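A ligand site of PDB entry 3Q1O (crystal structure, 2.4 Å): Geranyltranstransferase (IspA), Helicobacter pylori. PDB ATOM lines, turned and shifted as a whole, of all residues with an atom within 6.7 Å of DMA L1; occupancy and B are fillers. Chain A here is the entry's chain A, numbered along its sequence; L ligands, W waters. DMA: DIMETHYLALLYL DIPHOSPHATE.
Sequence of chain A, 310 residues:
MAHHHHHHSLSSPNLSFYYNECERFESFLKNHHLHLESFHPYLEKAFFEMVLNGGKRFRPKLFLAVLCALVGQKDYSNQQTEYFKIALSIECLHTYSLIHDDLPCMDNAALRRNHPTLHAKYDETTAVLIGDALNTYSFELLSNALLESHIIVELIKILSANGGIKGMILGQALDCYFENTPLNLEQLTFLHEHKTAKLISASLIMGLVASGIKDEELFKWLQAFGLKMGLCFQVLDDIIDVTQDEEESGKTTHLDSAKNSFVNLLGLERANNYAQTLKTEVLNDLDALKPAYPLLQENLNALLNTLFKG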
ATOM      1  N   GLY A  54      21.415  24.194 -12.316  1.00  0.00           N
ATOM      2  CA  GLY A  54      20.016  24.410 -11.974  1.00  0.00           C
ATOM      3  C   GLY A  54      19.163  23.245 -12.406  1.00  0.00           C
ATOM      4  O   GLY A  54      19.672  22.143 -12.630  1.00  0.00           O
ATOM      5  N   GLY A  55      17.866  23.497 -12.523  1.00  0.00           N
ATOM      6  CA  GLY A  55      16.902  22.489 -12.905  1.00  0.00           C
ATOM      7  C   GLY A  55      15.824  22.413 -11.853  1.00  0.00           C
ATOM      8  O   GLY A  55      16.087  22.710 -10.689  1.00  0.00           O
ATOM      9  N   LYS A  56      14.624  22.026 -12.251  1.00  0.00           N
ATOM     10  CA  LYS A  56      13.501  21.899 -11.331  1.00  0.00           C
ATOM     11  C   LYS A  56      13.604  20.627 -10.486  1.00  0.00           C
ATOM     12  O   LYS A  56      12.894  20.498  -9.484  1.00  0.00           O
ATOM     13  CB  LYS A  56      12.161  21.899 -12.075  1.00  0.00           C
ATOM     14  CG  LYS A  56      11.804  23.227 -12.736  1.00  0.00           C
ATOM     15  CD  LYS A  56      10.504  23.119 -13.534  1.00  0.00           C
ATOM     16  CE  LYS A  56      10.658  22.248 -14.787  1.00  0.00           C
ATOM     17  NZ  LYS A  56      11.749  22.721 -15.681  1.00  0.00           N
ATOM     18  N   ARG A  57      14.448  19.695 -10.913  1.00  0.00           N
ATOM     19  CA  ARG A  57      14.631  18.384 -10.265  1.00  0.00           C
ATOM     20  C   ARG A  57      13.326  17.604 -10.300  1.00  0.00           C
ATOM     21  O   ARG A  57      13.022  16.853  -9.375  1.00  0.00           O
ATOM     22  CB  ARG A  57      15.152  18.510  -8.824  1.00  0.00           C
ATOM     23  CG  ARG A  57      16.669  18.619  -8.626  1.00  0.00           C
ATOM     24  CD  ARG A  57      17.376  19.309  -9.769  1.00  0.00           C
ATOM     25  NE  ARG A  57      18.523  20.084  -9.332  1.00  0.00           N
ATOM     26  CZ  ARG A  57      19.627  20.232 -10.045  1.00  0.00           C
ATOM     27  NH1 ARG A  57      20.623  20.979  -9.567  1.00  0.00           N
ATOM     28  NH2 ARG A  57      19.752  19.633 -11.223  1.00  0.00           N
ATOM     29  N   PHE A  58      12.563  17.791 -11.385  1.00  0.00           N
ATOM     30  CA  PHE A  58      11.218  17.218 -11.502  1.00  0.00           C
ATOM     31  C   PHE A  58      11.226  15.714 -11.391  1.00  0.00           C
ATOM     32  O   PHE A  58      10.382  15.128 -10.717  1.00  0.00           O
ATOM     33  CB  PHE A  58      10.545  17.659 -12.818  1.00  0.00           C
ATOM     34  CG  PHE A  58       9.137  17.140 -12.970  1.00  0.00           C
ATOM     35  CD1 PHE A  58       8.162  17.394 -12.001  1.00  0.00           C
ATOM     36  CD2 PHE A  58       8.776  16.415 -14.105  1.00  0.00           C
ATOM     37  CE1 PHE A  58       6.854  16.913 -12.159  1.00  0.00           C
ATOM     38  CE2 PHE A  58       7.460  15.952 -14.267  1.00  0.00           C
ATOM     39  CZ  PHE A  58       6.513  16.196 -13.290  1.00  0.00           C
ATOM     40  N   ARG A  59      12.196  15.081 -12.055  1.00  0.00           N
ATOM     41  CA  ARG A  59      12.299  13.631 -12.056  1.00  0.00           C
ATOM     42  C   ARG A  59      12.734  13.030 -10.690  1.00  0.00           C
ATOM     43  O   ARG A  59      12.108  12.080 -10.228  1.00  0.00           O
ATOM     44  CB  ARG A  59      13.146  13.151 -13.238  1.00  0.00           C
ATOM     45  CG  ARG A  59      12.482  13.437 -14.572  1.00  0.00           C
ATOM     46  CD  ARG A  59      13.486  13.729 -15.656  1.00  0.00           C
ATOM     47  NE  ARG A  59      12.839  14.267 -16.852  1.00  0.00           N
ATOM     48  CZ  ARG A  59      12.652  15.570 -17.087  1.00  0.00           C
ATOM     49  NH1 ARG A  59      12.058  15.969 -18.211  1.00  0.00           N
ATOM     50  NH2 ARG A  59      13.031  16.473 -16.197  1.00  0.00           N
ATOM     51  N   GLU A  91      18.794  12.167 -12.439  1.00  0.00           N
ATOM     52  CA  GLU A  91      19.135  13.539 -12.791  1.00  0.00           C
ATOM     53  C   GLU A  91      20.370  13.617 -13.688  1.00  0.00           C
ATOM     54  O   GLU A  91      20.413  14.439 -14.616  1.00  0.00           O
ATOM     55  CB  GLU A  91      19.292  14.393 -11.529  1.00  0.00           C
ATOM     56  CG  GLU A  91      19.462  15.900 -11.779  1.00  0.00           C
ATOM     57  CD  GLU A  91      18.247  16.568 -12.434  1.00  0.00           C
ATOM     58  OE1 GLU A  91      17.143  15.973 -12.444  1.00  0.00           O
ATOM     59  OE2 GLU A  91      18.394  17.696 -12.927  1.00  0.00           O
ATOM     60  N   HIS A  94      19.215  12.513 -17.147  1.00  0.00           N
ATOM     61  CA  HIS A  94      18.450  13.637 -17.667  1.00  0.00           C
ATOM     62  C   HIS A  94      19.366  14.792 -18.120  1.00  0.00           C
ATOM     63  O   HIS A  94      19.220  15.292 -19.242  1.00  0.00           O
ATOM     64  CB  HIS A  94      17.407  14.119 -16.646  1.00  0.00           C
ATOM     65  CG  HIS A  94      16.715  15.380 -17.044  1.00  0.00           C
ATOM     66  ND1 HIS A  94      16.042  15.509 -18.240  1.00  0.00           N
ATOM     67  CD2 HIS A  94      16.604  16.575 -16.419  1.00  0.00           C
ATOM     68  CE1 HIS A  94      15.552  16.740 -18.329  1.00  0.00           C
ATOM     69  NE2 HIS A  94      15.879  17.396 -17.240  1.00  0.00           N
ATOM     70  N   THR A  95      20.323  15.174 -17.273  1.00  0.00           N
ATOM     71  CA  THR A  95      21.302  16.219 -17.604  1.00  0.00           C
ATOM     72  C   THR A  95      22.151  15.882 -18.839  1.00  0.00           C
ATOM     73  O   THR A  95      22.386  16.746 -19.683  1.00  0.00           O
ATOM     74  CB  THR A  95      22.231  16.514 -16.397  1.00  0.00           C
ATOM     75  OG1 THR A  95      21.432  16.849 -15.250  1.00  0.00           O
ATOM     76  CG2 THR A  95      23.152  17.664 -16.702  1.00  0.00           C
ATOM     77  N   SER A  97      21.209  14.136 -21.405  1.00  0.00           N
ATOM     78  CA  SER A  97      20.369  14.312 -22.593  1.00  0.00           C
ATOM     79  C   SER A  97      20.240  15.778 -22.976  1.00  0.00           C
ATOM     80  O   SER A  97      20.232  16.087 -24.155  1.00  0.00           O
ATOM     81  CB  SER A  97      18.986  13.703 -22.393  1.00  0.00           C
ATOM     82  OG  SER A  97      18.209  14.494 -21.492  1.00  0.00           O
ATOM     83  N   LEU A  98      20.137  16.652 -21.967  1.00  0.00           N
ATOM     84  CA  LEU A  98      20.129  18.103 -22.159  1.00  0.00           C
ATOM     85  C   LEU A  98      21.398  18.598 -22.853  1.00  0.00           C
ATOM     86  O   LEU A  98      21.323  19.350 -23.832  1.00  0.00           O
ATOM     87  CB  LEU A  98      19.951  18.839 -20.833  1.00  0.00           C
ATOM     88  CG  LEU A  98      18.704  18.568 -19.987  1.00  0.00           C
ATOM     89  CD1 LEU A  98      18.669  19.460 -18.751  1.00  0.00           C
ATOM     90  CD2 LEU A  98      17.451  18.762 -20.801  1.00  0.00           C
ATOM     91  N   ARG A 112      21.475  27.100 -21.090  1.00  0.00           N
ATOM     92  CA  ARG A 112      20.586  26.208 -20.334  1.00  0.00           C
ATOM     93  C   ARG A 112      20.772  26.361 -18.830  1.00  0.00           C
ATOM     94  O   ARG A 112      21.899  26.496 -18.355  1.00  0.00           O
ATOM     95  CB  ARG A 112      20.738  24.734 -20.726  1.00  0.00           C
ATOM     96  CG  ARG A 112      19.534  23.926 -20.238  1.00  0.00           C
ATOM     97  CD  ARG A 112      19.593  22.493 -20.586  1.00  0.00           C
ATOM     98  NE  ARG A 112      19.195  22.199 -21.965  1.00  0.00           N
ATOM     99  CZ  ARG A 112      17.951  22.010 -22.385  1.00  0.00           C
ATOM    100  NH1 ARG A 112      16.910  22.124 -21.560  1.00  0.00           N
ATOM    101  NH2 ARG A 112      17.740  21.717 -23.661  1.00  0.00           N
ATOM    102  N   ARG A 113      19.650  26.328 -18.110  1.00  0.00           N
ATOM    103  CA  ARG A 113      19.601  26.443 -16.646  1.00  0.00           C
ATOM    104  C   ARG A 113      20.267  27.745 -16.163  1.00  0.00           C
ATOM    105  O   ARG A 113      21.015  27.747 -15.179  1.00  0.00           O
ATOM    106  CB  ARG A 113      20.187  25.177 -15.973  1.00  0.00           C
ATOM    107  CG  ARG A 113      19.422  23.884 -16.264  1.00  0.00           C
ATOM    108  CD  ARG A 113      20.205  22.625 -15.870  1.00  0.00           C
ATOM    109  NE  ARG A 113      19.347  21.434 -15.827  1.00  0.00           N
ATOM    110  CZ  ARG A 113      19.686  20.253 -15.300  1.00  0.00           C
ATOM    111  NH1 ARG A 113      20.875  20.054 -14.760  1.00  0.00           N
ATOM    112  NH2 ARG A 113      18.820  19.255 -15.314  1.00  0.00           N
ATOM    113  N   LYS A 195      10.552  10.808 -26.332  1.00  0.00           N
ATOM    114  CA  LYS A 195      11.473  11.880 -25.980  1.00  0.00           C
ATOM    115  C   LYS A 195      11.399  12.321 -24.499  1.00  0.00           C
ATOM    116  O   LYS A 195      12.440  12.580 -23.879  1.00  0.00           O
ATOM    117  CB  LYS A 195      11.189  13.086 -26.889  1.00  0.00           C
ATOM    118  CG  LYS A 195      12.182  14.214 -26.826  1.00  0.00           C
ATOM    119  CD  LYS A 195      11.814  15.341 -27.784  1.00  0.00           C
ATOM    120  CE  LYS A 195      10.672  16.197 -27.232  1.00  0.00           C
ATOM    121  NZ  LYS A 195      10.633  17.533 -27.876  1.00  0.00           N
ATOM    122  N   THR A 196      10.196  12.373 -23.931  1.00  0.00           N
ATOM    123  CA  THR A 196       9.995  12.998 -22.618  1.00  0.00           C
ATOM    124  C   THR A 196       9.281  12.126 -21.573  1.00  0.00           C
ATOM    125  O   THR A 196       9.711  12.067 -20.416  1.00  0.00           O
ATOM    126  CB  THR A 196       9.270  14.347 -22.788  1.00  0.00           C
ATOM    127  OG1 THR A 196      10.049  15.164 -23.667  1.00  0.00           O
ATOM    128  CG2 THR A 196       9.095  15.074 -21.460  1.00  0.00           C
ATOM    129  N   PHE A 233       3.638  17.156 -19.767  1.00  0.00           N
ATOM    130  CA  PHE A 233       4.858  17.898 -19.442  1.00  0.00           C
ATOM    131  C   PHE A 233       5.488  18.527 -20.705  1.00  0.00           C
ATOM    132  O   PHE A 233       5.813  19.716 -20.708  1.00  0.00           O
ATOM    133  CB  PHE A 233       5.857  16.994 -18.724  1.00  0.00           C
ATOM    134  CG  PHE A 233       7.078  17.722 -18.190  1.00  0.00           C
ATOM    135  CD1 PHE A 233       8.264  17.766 -18.923  1.00  0.00           C
ATOM    136  CD2 PHE A 233       7.039  18.337 -16.953  1.00  0.00           C
ATOM    137  CE1 PHE A 233       9.375  18.429 -18.433  1.00  0.00           C
ATOM    138  CE2 PHE A 233       8.157  19.004 -16.458  1.00  0.00           C
ATOM    139  CZ  PHE A 233       9.331  19.052 -17.198  1.00  0.00           C
ATOM    140  N   GLN A 234       5.631  17.733 -21.766  1.00  0.00           N
ATOM    141  CA  GLN A 234       6.222  18.208 -23.009  1.00  0.00           C
ATOM    142  C   GLN A 234       5.356  19.207 -23.778  1.00  0.00           C
ATOM    143  O   GLN A 234       5.872  20.126 -24.411  1.00  0.00           O
ATOM    144  CB  GLN A 234       6.602  17.026 -23.917  1.00  0.00           C
ATOM    145  CG  GLN A 234       7.442  17.409 -25.130  1.00  0.00           C
ATOM    146  CD  GLN A 234       8.681  18.205 -24.797  1.00  0.00           C
ATOM    147  OE1 GLN A 234       9.482  17.805 -23.957  1.00  0.00           O
ATOM    148  NE2 GLN A 234       8.854  19.341 -25.476  1.00  0.00           N
ATOM    149  N   ASP A 237       5.910  22.311 -22.143  1.00  0.00           N
ATOM    150  CA  ASP A 237       7.256  22.754 -22.503  1.00  0.00           C
ATOM    151  C   ASP A 237       7.261  23.417 -23.878  1.00  0.00           C
ATOM    152  O   ASP A 237       7.949  24.413 -24.077  1.00  0.00           O
ATOM    153  CB  ASP A 237       8.259  21.590 -22.478  1.00  0.00           C
ATOM    154  CG  ASP A 237       9.681  22.035 -22.776  1.00  0.00           C
ATOM    155  OD1 ASP A 237      10.282  22.729 -21.926  1.00  0.00           O
ATOM    156  OD2 ASP A 237      10.205  21.705 -23.863  1.00  0.00           O
ATOM    157  N   ILE A 240       5.911  26.761 -23.383  1.00  0.00           N
ATOM    158  CA  ILE A 240       6.934  27.571 -22.695  1.00  0.00           C
ATOM    159  C   ILE A 240       7.819  28.347 -23.684  1.00  0.00           C
ATOM    160  O   ILE A 240       8.103  29.521 -23.462  1.00  0.00           O
ATOM    161  CB  ILE A 240       7.769  26.695 -21.695  1.00  0.00           C
ATOM    162  CG1 ILE A 240       7.053  26.628 -20.343  1.00  0.00           C
ATOM    163  CG2 ILE A 240       9.199  27.233 -21.498  1.00  0.00           C
ATOM    164  CD1 ILE A 240       7.609  25.584 -19.391  1.00  0.00           C
ATOM    165  N   SER A 249      12.764  31.096 -18.600  1.00  0.00           N
ATOM    166  CA  SER A 249      12.921  29.672 -18.932  1.00  0.00           C
ATOM    167  C   SER A 249      14.286  29.114 -18.560  1.00  0.00           C
ATOM    168  O   SER A 249      14.421  27.917 -18.307  1.00  0.00           O
ATOM    169  CB  SER A 249      12.643  29.419 -20.429  1.00  0.00           C
ATOM    170  OG  SER A 249      13.690  29.918 -21.240  1.00  0.00           O
ATOM    171  N   LYS A 251      16.763  28.960 -20.580  1.00  0.00           N
ATOM    172  CA  LYS A 251      17.287  28.265 -21.760  1.00  0.00           C
ATOM    173  C   LYS A 251      16.944  29.001 -23.040  1.00  0.00           C
ATOM    174  O   LYS A 251      15.991  29.799 -23.065  1.00  0.00           O
ATOM    175  CB  LYS A 251      16.768  26.821 -21.808  1.00  0.00           C
ATOM    176  CG  LYS A 251      15.242  26.703 -21.805  1.00  0.00           C
ATOM    177  CD  LYS A 251      14.797  25.260 -21.921  1.00  0.00           C
ATOM    178  CE  LYS A 251      13.281  25.165 -22.064  1.00  0.00           C
ATOM    179  NZ  LYS A 251      12.784  23.772 -21.855  1.00  0.00           N
HETATM  180  C1  DMA L   1      13.857  19.803 -20.170  1.00  0.00           C
HETATM  181  O1  DMA L   1      13.505  19.315 -18.873  1.00  0.00           O
HETATM  182  C2  DMA L   1      13.706  18.520 -20.953  1.00  0.00           C
HETATM  183  C3  DMA L   1      12.549  18.159 -21.536  1.00  0.00           C
HETATM  184  C4  DMA L   1      11.330  19.043 -21.501  1.00  0.00           C
HETATM  185  C5  DMA L   1      12.495  16.842 -22.254  1.00  0.00           C
HETATM  186  PA  DMA L   1      13.101  20.213 -17.604  1.00  0.00           P
HETATM  187  O1A DMA L   1      12.900  19.265 -16.440  1.00  0.00           O
HETATM  188  O2A DMA L   1      12.000  21.151 -18.026  1.00  0.00           O
HETATM  189  O3A DMA L   1      14.452  21.058 -17.383  1.00  0.00           O
HETATM  190  PB  DMA L   1      15.300  21.051 -16.019  1.00  0.00           P
HETATM  191  O1B DMA L   1      16.374  22.077 -16.312  1.00  0.00           O
HETATM  192  O2B DMA L   1      14.321  21.426 -14.914  1.00  0.00           O
HETATM  193  O3B DMA L   1      15.807  19.639 -15.891  1.00  0.00           O
HETATM  194  C1  DMA L   2      14.599  17.701 -25.414  1.00  0.00           C
HETATM  195  O1  DMA L   2      13.401  18.162 -26.044  1.00  0.00           O
HETATM  196  C2  DMA L   2      14.539  16.243 -25.056  1.00  0.00           C
HETATM  197  C3  DMA L   2      15.461  15.708 -24.244  1.00  0.00           C
HETATM  198  C4  DMA L   2      16.582  16.536 -23.681  1.00  0.00           C
HETATM  199  C5  DMA L   2      15.384  14.250 -23.900  1.00  0.00           C
HETATM  200  PA  DMA L   2      13.363  19.734 -26.370  1.00  0.00           P
HETATM  201  O1A DMA L   2      14.552  20.003 -27.264  1.00  0.00           O
HETATM  202  O2A DMA L   2      11.975  20.121 -26.812  1.00  0.00           O
HETATM  203  O3A DMA L   2      13.637  20.324 -24.888  1.00  0.00           O
HETATM  204  PB  DMA L   2      14.147  21.812 -24.559  1.00  0.00           P
HETATM  205  O1B DMA L   2      14.272  21.775 -23.054  1.00  0.00           O
HETATM  206  O2B DMA L   2      15.439  21.948 -25.313  1.00  0.00           O
HETATM  207  O3B DMA L   2      13.030  22.704 -25.050  1.00  0.00           O
HETATM  208  O   HOH W   1      16.244  19.158 -13.122  1.00  0.00           O
HETATM  209  O   HOH W   2      15.756  24.690 -15.620  1.00  0.00           O
HETATM  210  O   HOH W   3       9.770  22.267 -19.343  1.00  0.00           O
HETATM  211  O   HOH W   4      16.014  23.271 -19.001  1.00  0.00           O
HETATM  212  O   HOH W   5      13.286  23.496 -19.121  1.00  0.00           O
HETATM  213  O   HOH W   6      13.389  19.089 -13.995  1.00  0.00           O
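OG of Ser 97 sits at hydrogen-bond distance from O of His 94 (2.6 Å).
The side-chain carboxylate (OE2) of Glu 91 is in salt-bridge range of the guanidinium group (NH2) of Arg 113, 2.9 Å away.
O of Gly 54 is in hydrogen-bond range of NH1 of Arg 113 (3.2 Å).
A ring nitrogen (NE2) of His 94 lies within hydrogen-bond range of the guanidinium group of Arg 59, 3.2 Å away.
The side-chain amide nitrogen (NE2) of Gln 234 lies within hydrogen-bond range of the side-chain carboxylate (OD2) of Asp 237, at 3.2 Å.
The side-chain amide nitrogen of Gln 234 sits close to the side-chain amino group of Lys 195.
OD1 of Asp 237 lies within salt-bridge range of NZ of Lys 251.
OG1 of Thr 95 sits at hydrogen-bond distance from NH1 of Arg 113 (3.3 Å).
Water W3 bridges OD1 of Asp 237 (2.7 Å) and O2A of DMA L1 (2.8 Å).
Water W5 bridges the side-chain amino group (NZ) of Lys 251 and an oxygen (O2A) of DMA L1.
Water W4 bridges the guanidinium group (NH1) of Arg 112 and an oxygen (O1B) of DMA L1.
Gly 55 touches DMA L1 (CA to O2B, 3.4 Å).
CD2 of Leu 98 touches C2 of DMA L1, at 3.8 Å.
OG1 of Thr 196 touches C5 of DMA L1 (3.3 Å).
Phe 233 touches DMA L1 (CZ to O2A, 3.5 Å).
Gln 234 touches DMA L1 (OE1 to C4, 3.3 Å).
Asp 237 touches DMA L1 (CG to C4, 3.6 Å).
Hydrophobic or aromatic side chains within 4 Å of DMA L1: His 94, Leu 98 and Phe 233.
Of the 21 residues printed, 10 come within 4 Å of DMA L1.
O2A of DMA L2 lies within salt-bridge range of NZ of Lys 195 (3.1 Å).
O2A of DMA L2 sits at hydrogen-bond distance from NE2 of Gln 234 (3.5 Å).
The guanidinium group (NE) of Arg 113 is in salt-bridge range of an oxygen (O1B) of DMA L1, 3.1 Å away.
NH2 of Arg 59 lies within salt-bridge range of O1A of DMA L1 (2.8 Å).
O1B of DMA L2 is in salt-bridge range of NZ of Lys 251 (2.8 Å).
O2B of DMA L1 is in hydrogen-bond range of N of Lys 56 (2.7 Å).
NH1 of Arg 112 lies within salt-bridge range of O1B of DMA L2 (3.1 Å).
O2A of DMA L1 is in salt-bridge range of NZ of Lys 56, at 2.8 Å.
An oxygen (O3B) of DMA L1 sits at hydrogen-bond distance from a ring nitrogen (NE2) of His 94 (2.6 Å).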
